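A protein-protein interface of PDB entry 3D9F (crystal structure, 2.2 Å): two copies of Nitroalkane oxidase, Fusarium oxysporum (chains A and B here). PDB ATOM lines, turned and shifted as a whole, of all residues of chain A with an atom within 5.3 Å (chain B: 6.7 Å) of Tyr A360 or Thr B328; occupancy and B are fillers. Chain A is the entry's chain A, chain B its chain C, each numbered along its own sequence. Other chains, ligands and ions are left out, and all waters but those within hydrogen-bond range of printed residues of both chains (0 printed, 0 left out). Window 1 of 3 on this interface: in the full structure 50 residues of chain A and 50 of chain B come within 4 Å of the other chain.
The backbone carbonyl oxygen (O) of Arg B325 is in hydrogen-bond range of the side-chain hydroxyl (OG1) of Thr B328 (3.0 Å).
O of Arg A325 sits at hydrogen-bond distance from OG1 of Thr A328.
The side-chain hydroxyl of Thr A328 is in hydrogen-bond range of the side-chain hydroxyl of Tyr A360, 2.5 Å away.
The guanidinium group (NH1) of Arg B330 is in salt-bridge range of the side-chain carboxylate (OE1) of Glu B327.
The backbone carbonyl oxygen (O) of Ile A324 lies within hydrogen-bond range of the side-chain hydroxyl (OG1) of Thr A328 (2.8 Å).
The side-chain hydroxyl (OG1) of Thr B328 sits at hydrogen-bond distance from the side-chain hydroxyl (OH) of Tyr B360.
Among the printed residues, pairs that only touch across the chains: Gln A356 with Glu B327 (3.2 Å), Ile A324 with Tyr B360 (3.3 Å), Tyr A360 with Ile B324 (3.4 Å), Gln A356 with Lys B323 (3.6 Å), Leu A332 with Leu B331 (3.6 Å), Tyr A360 with Tyr B360 (3.7 Å), Leu A332 with Glu B327 (3.7 Å), Thr A328 with Leu B332 (3.7 Å), Gln A356 with Ile B324 (3.8 Å), Tyr A360 with Thr B328 (3.9 Å) and Leu A332 with Thr B328 (3.9 Å).
Printed residues of chain B within 4 Å of Ile A324: Tyr B360 (3.3 Å).
Of the printed residues of chain B, Tyr A360 touches Ile B324 (3.4 Å), Thr B328 (3.9 Å) and Tyr B360 (3.7 Å).
Of the printed residues of chain A, Glu B327 touches Leu A332 (3.7 Å) and Gln A356 (3.2 Å).
Thr B328 touches just these residues of chain A: Leu A332 and Tyr A360.
Ser B329 touches none of the printed residues of chain A.
Printed residues of chain A within 4 Å of Leu B331: Leu A332 (3.6 Å).
The nearest residue of chain B that does not touch Tyr A360 is Arg B325 (6.0 Å).
The nearest printed residue of chain A that does not touch Tyr B360 is Thr A328 (4.02 Å).
Of the 15 printed residues of chain B, 7 touch a printed residue of chain A.
Hydrophobic or aromatic side chains of chain B within 4 Å of the printed part of chain A: Ile B324, Leu B331, Leu B332 and Tyr B360.
Ile A324 touches Tyr B360, and with the chains exchanged Tyr A360 touches Ile B324.
Thr A328 touches Leu B332, and with the chains exchanged Leu A332 touches Thr B328.
Tyr A360 touches Thr B328, but with the chains exchanged Thr A328 does not touch Tyr B360 (4.02 Å).
Tyr B360 touches its own counterpart, Tyr A360.
Of the 11 pairs that touch across the chains among the printed residues, 5 have their exchanged pair printed and touching as well.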
ATOM      1  N   ILE A 324      10.241 -23.659  36.015  1.00  0.00           N
ATOM      2  CA  ILE A 324       9.317 -24.695  35.589  1.00  0.00           C
ATOM      3  C   ILE A 324       9.132 -24.695  34.071  1.00  0.00           C
ATOM      4  O   ILE A 324       9.072 -25.761  33.451  1.00  0.00           O
ATOM      5  CB  ILE A 324       7.959 -24.565  36.329  1.00  0.00           C
ATOM      6  CG1 ILE A 324       8.138 -24.960  37.801  1.00  0.00           C
ATOM      7  CG2 ILE A 324       6.867 -25.393  35.636  1.00  0.00           C
ATOM      8  CD1 ILE A 324       6.958 -24.611  38.709  1.00  0.00           C
ATOM      9  N   ARG A 325       9.038 -23.498  33.487  1.00  0.00           N
ATOM     10  CA  ARG A 325       8.918 -23.339  32.028  1.00  0.00           C
ATOM     11  C   ARG A 325      10.118 -23.883  31.279  1.00  0.00           C
ATOM     12  O   ARG A 325       9.973 -24.534  30.247  1.00  0.00           O
ATOM     13  CB  ARG A 325       8.725 -21.878  31.640  1.00  0.00           C
ATOM     14  CG  ARG A 325       7.347 -21.365  31.949  1.00  0.00           C
ATOM     15  CD  ARG A 325       7.341 -19.871  31.942  1.00  0.00           C
ATOM     16  NE  ARG A 325       6.080 -19.378  32.492  1.00  0.00           N
ATOM     17  CZ  ARG A 325       5.976 -18.301  33.266  1.00  0.00           C
ATOM     18  NH1 ARG A 325       4.777 -17.948  33.709  1.00  0.00           N
ATOM     19  NH2 ARG A 325       7.062 -17.591  33.614  1.00  0.00           N
ATOM     20  N   THR A 328      10.285 -27.944  31.907  1.00  0.00           N
ATOM     21  CA  THR A 328       9.302 -28.618  31.083  1.00  0.00           C
ATOM     22  C   THR A 328       9.643 -28.507  29.593  1.00  0.00           C
ATOM     23  O   THR A 328       9.466 -29.467  28.846  1.00  0.00           O
ATOM     24  CB  THR A 328       7.844 -28.144  31.387  1.00  0.00           C
ATOM     25  OG1 THR A 328       7.732 -26.713  31.246  1.00  0.00           O
ATOM     26  CG2 THR A 328       7.442 -28.560  32.790  1.00  0.00           C
ATOM     27  N   SER A 329      10.126 -27.337  29.175  1.00  0.00           N
ATOM     28  CA  SER A 329      10.527 -27.097  27.791  1.00  0.00           C
ATOM     29  C   SER A 329      11.649 -28.026  27.316  1.00  0.00           C
ATOM     30  O   SER A 329      11.559 -28.613  26.215  1.00  0.00           O
ATOM     31  CB  SER A 329      10.971 -25.646  27.598  1.00  0.00           C
ATOM     32  OG  SER A 329       9.875 -24.762  27.602  1.00  0.00           O
ATOM     33  N   LEU A 332      10.541 -31.601  26.864  1.00  0.00           N
ATOM     34  CA  LEU A 332       9.663 -31.767  25.716  1.00  0.00           C
ATOM     35  C   LEU A 332      10.462 -31.765  24.402  1.00  0.00           C
ATOM     36  O   LEU A 332      10.097 -32.471  23.445  1.00  0.00           O
ATOM     37  CB  LEU A 332       8.568 -30.683  25.715  1.00  0.00           C
ATOM     38  CG  LEU A 332       7.460 -30.731  24.663  1.00  0.00           C
ATOM     39  CD1 LEU A 332       6.535 -32.015  24.785  1.00  0.00           C
ATOM     40  CD2 LEU A 332       6.619 -29.430  24.717  1.00  0.00           C
ATOM     41  N   MET A 355       5.032 -30.320  16.608  1.00  0.00           N
ATOM     42  CA  MET A 355       4.184 -29.137  16.699  1.00  0.00           C
ATOM     43  C   MET A 355       3.949 -28.722  18.154  1.00  0.00           C
ATOM     44  O   MET A 355       4.068 -27.550  18.459  1.00  0.00           O
ATOM     45  CB  MET A 355       2.830 -29.338  15.994  1.00  0.00           C
ATOM     46  CG  MET A 355       2.896 -29.735  14.510  1.00  0.00           C
ATOM     47  SD  MET A 355       3.761 -28.558  13.467  1.00  0.00           S
ATOM     48  CE  MET A 355       5.429 -29.235  13.413  1.00  0.00           C
ATOM     49  N   GLN A 356       3.610 -29.672  19.029  1.00  0.00           N
ATOM     50  CA  GLN A 356       3.432 -29.418  20.469  1.00  0.00           C
ATOM     51  C   GLN A 356       4.635 -28.683  21.035  1.00  0.00           C
ATOM     52  O   GLN A 356       4.486 -27.735  21.796  1.00  0.00           O
ATOM     53  CB  GLN A 356       3.369 -30.726  21.264  1.00  0.00           C
ATOM     54  CG  GLN A 356       2.070 -31.449  21.292  1.00  0.00           C
ATOM     55  CD  GLN A 356       2.164 -32.733  22.083  1.00  0.00           C
ATOM     56  OE1 GLN A 356       2.248 -33.812  21.518  1.00  0.00           O
ATOM     57  NE2 GLN A 356       2.199 -32.620  23.392  1.00  0.00           N
ATOM     58  N   THR A 357       5.821 -29.192  20.699  1.00  0.00           N
ATOM     59  CA  THR A 357       7.079 -28.699  21.223  1.00  0.00           C
ATOM     60  C   THR A 357       7.311 -27.238  20.797  1.00  0.00           C
ATOM     61  O   THR A 357       7.643 -26.386  21.618  1.00  0.00           O
ATOM     62  CB  THR A 357       8.224 -29.611  20.757  1.00  0.00           C
ATOM     63  OG1 THR A 357       7.897 -30.968  21.085  1.00  0.00           O
ATOM     64  CG2 THR A 357       9.520 -29.246  21.446  1.00  0.00           C
ATOM     65  N   LYS A 358       7.072 -26.962  19.525  1.00  0.00           N
ATOM     66  CA  LYS A 358       7.305 -25.656  18.984  1.00  0.00           C
ATOM     67  C   LYS A 358       6.346 -24.663  19.641  1.00  0.00           C
ATOM     68  O   LYS A 358       6.774 -23.592  20.087  1.00  0.00           O
ATOM     69  CB  LYS A 358       7.126 -25.656  17.451  1.00  0.00           C
ATOM     70  CG  LYS A 358       7.806 -24.474  16.724  1.00  0.00           C
ATOM     71  CD  LYS A 358       7.086 -23.146  16.932  1.00  0.00           C
ATOM     72  CE  LYS A 358       7.735 -22.006  16.141  1.00  0.00           C
ATOM     73  NZ  LYS A 358       6.854 -20.801  15.959  1.00  0.00           N
ATOM     74  N   ILE A 359       5.061 -25.030  19.702  1.00  0.00           N
ATOM     75  CA  ILE A 359       4.053 -24.175  20.320  1.00  0.00           C
ATOM     76  C   ILE A 359       4.402 -23.917  21.786  1.00  0.00           C
ATOM     77  O   ILE A 359       4.514 -22.771  22.198  1.00  0.00           O
ATOM     78  CB  ILE A 359       2.613 -24.760  20.177  1.00  0.00           C
ATOM     79  CG1 ILE A 359       2.216 -24.874  18.697  1.00  0.00           C
ATOM     80  CG2 ILE A 359       1.599 -23.911  20.927  1.00  0.00           C
ATOM     81  CD1 ILE A 359       1.087 -25.929  18.429  1.00  0.00           C
ATOM     82  N   TYR A 360       4.575 -24.966  22.574  1.00  0.00           N
ATOM     83  CA  TYR A 360       4.747 -24.768  24.008  1.00  0.00           C
ATOM     84  C   TYR A 360       6.030 -23.978  24.331  1.00  0.00           C
ATOM     85  O   TYR A 360       5.967 -22.945  25.000  1.00  0.00           O
ATOM     86  CB  TYR A 360       4.727 -26.094  24.782  1.00  0.00           C
ATOM     87  CG  TYR A 360       5.013 -25.931  26.274  1.00  0.00           C
ATOM     88  CD1 TYR A 360       4.007 -25.521  27.160  1.00  0.00           C
ATOM     89  CD2 TYR A 360       6.290 -26.192  26.798  1.00  0.00           C
ATOM     90  CE1 TYR A 360       4.252 -25.375  28.514  1.00  0.00           C
ATOM     91  CE2 TYR A 360       6.559 -26.049  28.151  1.00  0.00           C
ATOM     92  CZ  TYR A 360       5.536 -25.630  29.005  1.00  0.00           C
ATOM     93  OH  TYR A 360       5.791 -25.486  30.357  1.00  0.00           O
ATOM     94  N   THR A 361       7.179 -24.465  23.849  1.00  0.00           N
ATOM     95  CA  THR A 361       8.474 -23.892  24.218  1.00  0.00           C
ATOM     96  C   THR A 361       8.616 -22.425  23.811  1.00  0.00           C
ATOM     97  O   THR A 361       9.211 -21.631  24.549  1.00  0.00           O
ATOM     98  CB  THR A 361       9.638 -24.698  23.646  1.00  0.00           C
ATOM     99  OG1 THR A 361       9.575 -24.659  22.213  1.00  0.00           O
ATOM    100  CG2 THR A 361       9.584 -26.177  24.145  1.00  0.00           C
ATOM    101  N   THR A 362       8.049 -22.064  22.660  1.00  0.00           N
ATOM    102  CA  THR A 362       8.179 -20.716  22.143  1.00  0.00           C
ATOM    103  C   THR A 362       7.253 -19.711  22.830  1.00  0.00           C
ATOM    104  O   THR A 362       7.665 -18.574  23.087  1.00  0.00           O
ATOM    105  CB  THR A 362       8.084 -20.639  20.589  1.00  0.00           C
ATOM    106  OG1 THR A 362       6.750 -20.940  20.114  1.00  0.00           O
ATOM    107  CG2 THR A 362       9.122 -21.570  19.949  1.00  0.00           C
ATOM    108  N   ASP A 363       6.013 -20.119  23.116  1.00  0.00           N
ATOM    109  CA  ASP A 363       5.096 -19.283  23.899  1.00  0.00           C
ATOM    110  C   ASP A 363       5.613 -19.050  25.328  1.00  0.00           C
ATOM    111  O   ASP A 363       5.659 -17.923  25.831  1.00  0.00           O
ATOM    112  CB  ASP A 363       3.712 -19.916  23.970  1.00  0.00           C
ATOM    113  CG  ASP A 363       2.923 -19.744  22.682  1.00  0.00           C
ATOM    114  OD1 ASP A 363       1.914 -20.470  22.543  1.00  0.00           O
ATOM    115  OD2 ASP A 363       3.289 -18.902  21.817  1.00  0.00           O
ATOM    116  N   VAL A 364       5.983 -20.148  25.958  1.00  0.00           N
ATOM    117  CA  VAL A 364       6.444 -20.182  27.315  1.00  0.00           C
ATOM    118  C   VAL A 364       7.811 -19.439  27.516  1.00  0.00           C
ATOM    119  O   VAL A 364       8.079 -18.924  28.610  1.00  0.00           O
ATOM    120  CB  VAL A 364       6.344 -21.654  27.787  1.00  0.00           C
ATOM    121  CG1 VAL A 364       7.627 -22.248  28.322  1.00  0.00           C
ATOM    122  CG2 VAL A 364       5.097 -21.869  28.662  1.00  0.00           C
ATOM    123  N   ALA A 365       8.648 -19.359  26.469  1.00  0.00           N
ATOM    124  CA  ALA A 365       9.926 -18.614  26.560  1.00  0.00           C
ATOM    125  C   ALA A 365       9.737 -17.114  26.727  1.00  0.00           C
ATOM    126  O   ALA A 365      10.525 -16.447  27.437  1.00  0.00           O
ATOM    127  CB  ALA A 365      10.841 -18.898  25.351  1.00  0.00           C
ATOM    128  N   ILE B 284      -2.278 -36.124  36.325  1.00  0.00           N
ATOM    129  CA  ILE B 284      -2.292 -36.521  34.911  1.00  0.00           C
ATOM    130  C   ILE B 284      -3.424 -37.522  34.599  1.00  0.00           C
ATOM    131  O   ILE B 284      -4.082 -37.389  33.581  1.00  0.00           O
ATOM    132  CB  ILE B 284      -0.969 -37.143  34.444  1.00  0.00           C
ATOM    133  CG1 ILE B 284       0.172 -36.135  34.536  1.00  0.00           C
ATOM    134  CG2 ILE B 284      -1.097 -37.678  32.961  1.00  0.00           C
ATOM    135  CD1 ILE B 284       1.557 -36.786  34.487  1.00  0.00           C
ATOM    136  N   LYS B 323      -3.549 -31.212  25.682  1.00  0.00           N
ATOM    137  CA  LYS B 323      -2.563 -32.186  25.264  1.00  0.00           C
ATOM    138  C   LYS B 323      -1.135 -31.773  25.701  1.00  0.00           C
ATOM    139  O   LYS B 323      -0.397 -32.563  26.276  1.00  0.00           O
ATOM    140  CB  LYS B 323      -2.654 -32.367  23.726  1.00  0.00           C
ATOM    141  CG  LYS B 323      -1.866 -33.539  23.137  1.00  0.00           C
ATOM    142  CD  LYS B 323      -1.912 -34.826  23.972  1.00  0.00           C
ATOM    143  CE  LYS B 323      -1.695 -36.085  23.122  1.00  0.00           C
ATOM    144  NZ  LYS B 323      -0.530 -35.980  22.155  1.00  0.00           N
ATOM    145  N   ILE B 324      -0.773 -30.526  25.433  1.00  0.00           N
ATOM    146  CA  ILE B 324       0.528 -29.992  25.828  1.00  0.00           C
ATOM    147  C   ILE B 324       0.743 -30.076  27.335  1.00  0.00           C
ATOM    148  O   ILE B 324       1.782 -30.556  27.801  1.00  0.00           O
ATOM    149  CB  ILE B 324       0.679 -28.553  25.301  1.00  0.00           C
ATOM    150  CG1 ILE B 324       0.992 -28.635  23.796  1.00  0.00           C
ATOM    151  CG2 ILE B 324       1.755 -27.806  26.100  1.00  0.00           C
ATOM    152  CD1 ILE B 324       0.871 -27.335  23.019  1.00  0.00           C
ATOM    153  N   ARG B 325      -0.275 -29.675  28.099  1.00  0.00           N
ATOM    154  CA  ARG B 325      -0.214 -29.783  29.554  1.00  0.00           C
ATOM    155  C   ARG B 325       0.035 -31.192  30.024  1.00  0.00           C
ATOM    156  O   ARG B 325       0.847 -31.402  30.909  1.00  0.00           O
ATOM    157  CB  ARG B 325      -1.477 -29.242  30.209  1.00  0.00           C
ATOM    158  CG  ARG B 325      -1.733 -27.735  29.969  1.00  0.00           C
ATOM    159  CD  ARG B 325      -2.774 -27.216  30.964  1.00  0.00           C
ATOM    160  NE  ARG B 325      -3.789 -26.332  30.392  1.00  0.00           N
ATOM    161  CZ  ARG B 325      -3.574 -25.117  29.875  1.00  0.00           C
ATOM    162  NH1 ARG B 325      -2.354 -24.601  29.792  1.00  0.00           N
ATOM    163  NH2 ARG B 325      -4.599 -24.429  29.392  1.00  0.00           N
ATOM    164  N   LEU B 326      -0.681 -32.153  29.446  1.00  0.00           N
ATOM    165  CA  LEU B 326      -0.539 -33.558  29.806  1.00  0.00           C
ATOM    166  C   LEU B 326       0.854 -34.107  29.463  1.00  0.00           C
ATOM    167  O   LEU B 326       1.457 -34.814  30.257  1.00  0.00           O
ATOM    168  CB  LEU B 326      -1.624 -34.397  29.107  1.00  0.00           C
ATOM    169  CG  LEU B 326      -3.060 -34.220  29.650  1.00  0.00           C
ATOM    170  CD1 LEU B 326      -4.080 -34.886  28.733  1.00  0.00           C
ATOM    171  CD2 LEU B 326      -3.174 -34.751  31.091  1.00  0.00           C
ATOM    172  N   GLU B 327       1.341 -33.773  28.278  1.00  0.00           N
ATOM    173  CA  GLU B 327       2.602 -34.282  27.791  1.00  0.00           C
ATOM    174  C   GLU B 327       3.796 -33.736  28.582  1.00  0.00           C
ATOM    175  O   GLU B 327       4.662 -34.502  29.014  1.00  0.00           O
ATOM    176  CB  GLU B 327       2.744 -33.951  26.304  1.00  0.00           C
ATOM    177  CG  GLU B 327       3.987 -34.557  25.657  1.00  0.00           C
ATOM    178  CD  GLU B 327       3.948 -36.088  25.637  1.00  0.00           C
ATOM    179  OE1 GLU B 327       2.874 -36.648  25.300  1.00  0.00           O
ATOM    180  OE2 GLU B 327       4.999 -36.712  25.951  1.00  0.00           O
ATOM    181  N   THR B 328       3.843 -32.417  28.776  1.00  0.00           N
ATOM    182  CA  THR B 328       4.853 -31.807  29.656  1.00  0.00           C
ATOM    183  C   THR B 328       4.782 -32.376  31.070  1.00  0.00           C
ATOM    184  O   THR B 328       5.827 -32.648  31.684  1.00  0.00           O
ATOM    185  CB  THR B 328       4.699 -30.264  29.689  1.00  0.00           C
ATOM    186  OG1 THR B 328       3.334 -29.925  29.971  1.00  0.00           O
ATOM    187  CG2 THR B 328       5.066 -29.646  28.333  1.00  0.00           C
ATOM    188  N   SER B 329       3.567 -32.574  31.591  1.00  0.00           N
ATOM    189  CA  SER B 329       3.411 -33.070  32.954  1.00  0.00           C
ATOM    190  C   SER B 329       4.016 -34.458  33.129  1.00  0.00           C
ATOM    191  O   SER B 329       4.708 -34.730  34.127  1.00  0.00           O
ATOM    192  CB  SER B 329       1.943 -33.140  33.369  1.00  0.00           C
ATOM    193  OG  SER B 329       1.350 -31.859  33.408  1.00  0.00           O
ATOM    194  N   ARG B 330       3.723 -35.349  32.171  1.00  0.00           N
ATOM    195  CA  ARG B 330       4.179 -36.731  32.306  1.00  0.00           C
ATOM    196  C   ARG B 330       5.702 -36.794  32.215  1.00  0.00           C
ATOM    197  O   ARG B 330       6.340 -37.520  32.965  1.00  0.00           O
ATOM    198  CB  ARG B 330       3.510 -37.632  31.260  1.00  0.00           C
ATOM    199  CG  ARG B 330       3.786 -39.100  31.491  1.00  0.00           C
ATOM    200  CD  ARG B 330       3.313 -39.971  30.331  1.00  0.00           C
ATOM    201  NE  ARG B 330       1.858 -39.943  30.244  1.00  0.00           N
ATOM    202  CZ  ARG B 330       1.186 -39.338  29.275  1.00  0.00           C
ATOM    203  NH1 ARG B 330       1.836 -38.692  28.321  1.00  0.00           N
ATOM    204  NH2 ARG B 330      -0.143 -39.371  29.269  1.00  0.00           N
ATOM    205  N   LEU B 331       6.278 -36.025  31.298  1.00  0.00           N
ATOM    206  CA  LEU B 331       7.743 -35.956  31.144  1.00  0.00           C
ATOM    207  C   LEU B 331       8.406 -35.472  32.418  1.00  0.00           C
ATOM    208  O   LEU B 331       9.455 -35.989  32.819  1.00  0.00           O
ATOM    209  CB  LEU B 331       8.116 -35.006  30.005  1.00  0.00           C
ATOM    210  CG  LEU B 331       7.773 -35.486  28.600  1.00  0.00           C
ATOM    211  CD1 LEU B 331       7.921 -34.362  27.601  1.00  0.00           C
ATOM    212  CD2 LEU B 331       8.661 -36.651  28.245  1.00  0.00           C
ATOM    213  N   LEU B 332       7.781 -34.483  33.057  1.00  0.00           N
ATOM    214  CA  LEU B 332       8.281 -33.926  34.310  1.00  0.00           C
ATOM    215  C   LEU B 332       8.154 -34.917  35.456  1.00  0.00           C
ATOM    216  O   LEU B 332       9.076 -35.050  36.265  1.00  0.00           O
ATOM    217  CB  LEU B 332       7.603 -32.588  34.636  1.00  0.00           C
ATOM    218  CG  LEU B 332       8.163 -31.711  35.773  1.00  0.00           C
ATOM    219  CD1 LEU B 332       9.616 -31.254  35.533  1.00  0.00           C
ATOM    220  CD2 LEU B 332       7.260 -30.472  35.983  1.00  0.00           C
ATOM    221  N   VAL B 333       7.042 -35.644  35.517  1.00  0.00           N
ATOM    222  CA  VAL B 333       6.943 -36.710  36.504  1.00  0.00           C
ATOM    223  C   VAL B 333       8.040 -37.803  36.321  1.00  0.00           C
ATOM    224  O   VAL B 333       8.694 -38.215  37.295  1.00  0.00           O
ATOM    225  CB  VAL B 333       5.545 -37.327  36.549  1.00  0.00           C
ATOM    226  CG1 VAL B 333       5.534 -38.563  37.495  1.00  0.00           C
ATOM    227  CG2 VAL B 333       4.497 -36.268  36.966  1.00  0.00           C
ATOM    228  N   TYR B 360       3.784 -27.604  39.055  1.00  0.00           N
ATOM    229  CA  TYR B 360       3.356 -27.551  37.661  1.00  0.00           C
ATOM    230  C   TYR B 360       2.203 -28.511  37.360  1.00  0.00           C
ATOM    231  O   TYR B 360       1.156 -28.092  36.871  1.00  0.00           O
ATOM    232  CB  TYR B 360       4.513 -27.889  36.715  1.00  0.00           C
ATOM    233  CG  TYR B 360       4.098 -27.844  35.243  1.00  0.00           C
ATOM    234  CD1 TYR B 360       3.968 -26.631  34.587  1.00  0.00           C
ATOM    235  CD2 TYR B 360       3.842 -29.028  34.527  1.00  0.00           C
ATOM    236  CE1 TYR B 360       3.608 -26.578  33.268  1.00  0.00           C
ATOM    237  CE2 TYR B 360       3.465 -28.994  33.200  1.00  0.00           C
ATOM    238  CZ  TYR B 360       3.347 -27.769  32.573  1.00  0.00           C
ATOM    239  OH  TYR B 360       2.975 -27.714  31.258  1.00  0.00           O
ATOM    240  N   THR B 361       2.403 -29.790  37.643  1.00  0.00           N
ATOM    241  CA  THR B 361       1.430 -30.798  37.240  1.00  0.00           C
ATOM    242  C   THR B 361       0.055 -30.592  37.869  1.00  0.00           C
ATOM    243  O   THR B 361      -0.961 -30.783  37.188  1.00  0.00           O
ATOM    244  CB  THR B 361       1.908 -32.242  37.517  1.00  0.00           C
ATOM    245  OG1 THR B 361       1.993 -32.451  38.932  1.00  0.00           O
ATOM    246  CG2 THR B 361       3.272 -32.521  36.834  1.00  0.00           C
ATOM    247  N   VAL B 364      -1.641 -27.245  36.482  1.00  0.00           N
ATOM    248  CA  VAL B 364      -1.917 -27.410  35.064  1.00  0.00           C
ATOM    249  C   VAL B 364      -3.054 -28.439  34.817  1.00  0.00           C
ATOM    250  O   VAL B 364      -3.870 -28.260  33.915  1.00  0.00           O
ATOM    251  CB  VAL B 364      -0.529 -27.676  34.376  1.00  0.00           C
ATOM    252  CG1 VAL B 364      -0.318 -29.095  33.823  1.00  0.00           C
ATOM    253  CG2 VAL B 364      -0.151 -26.538  33.478  1.00  0.00           C
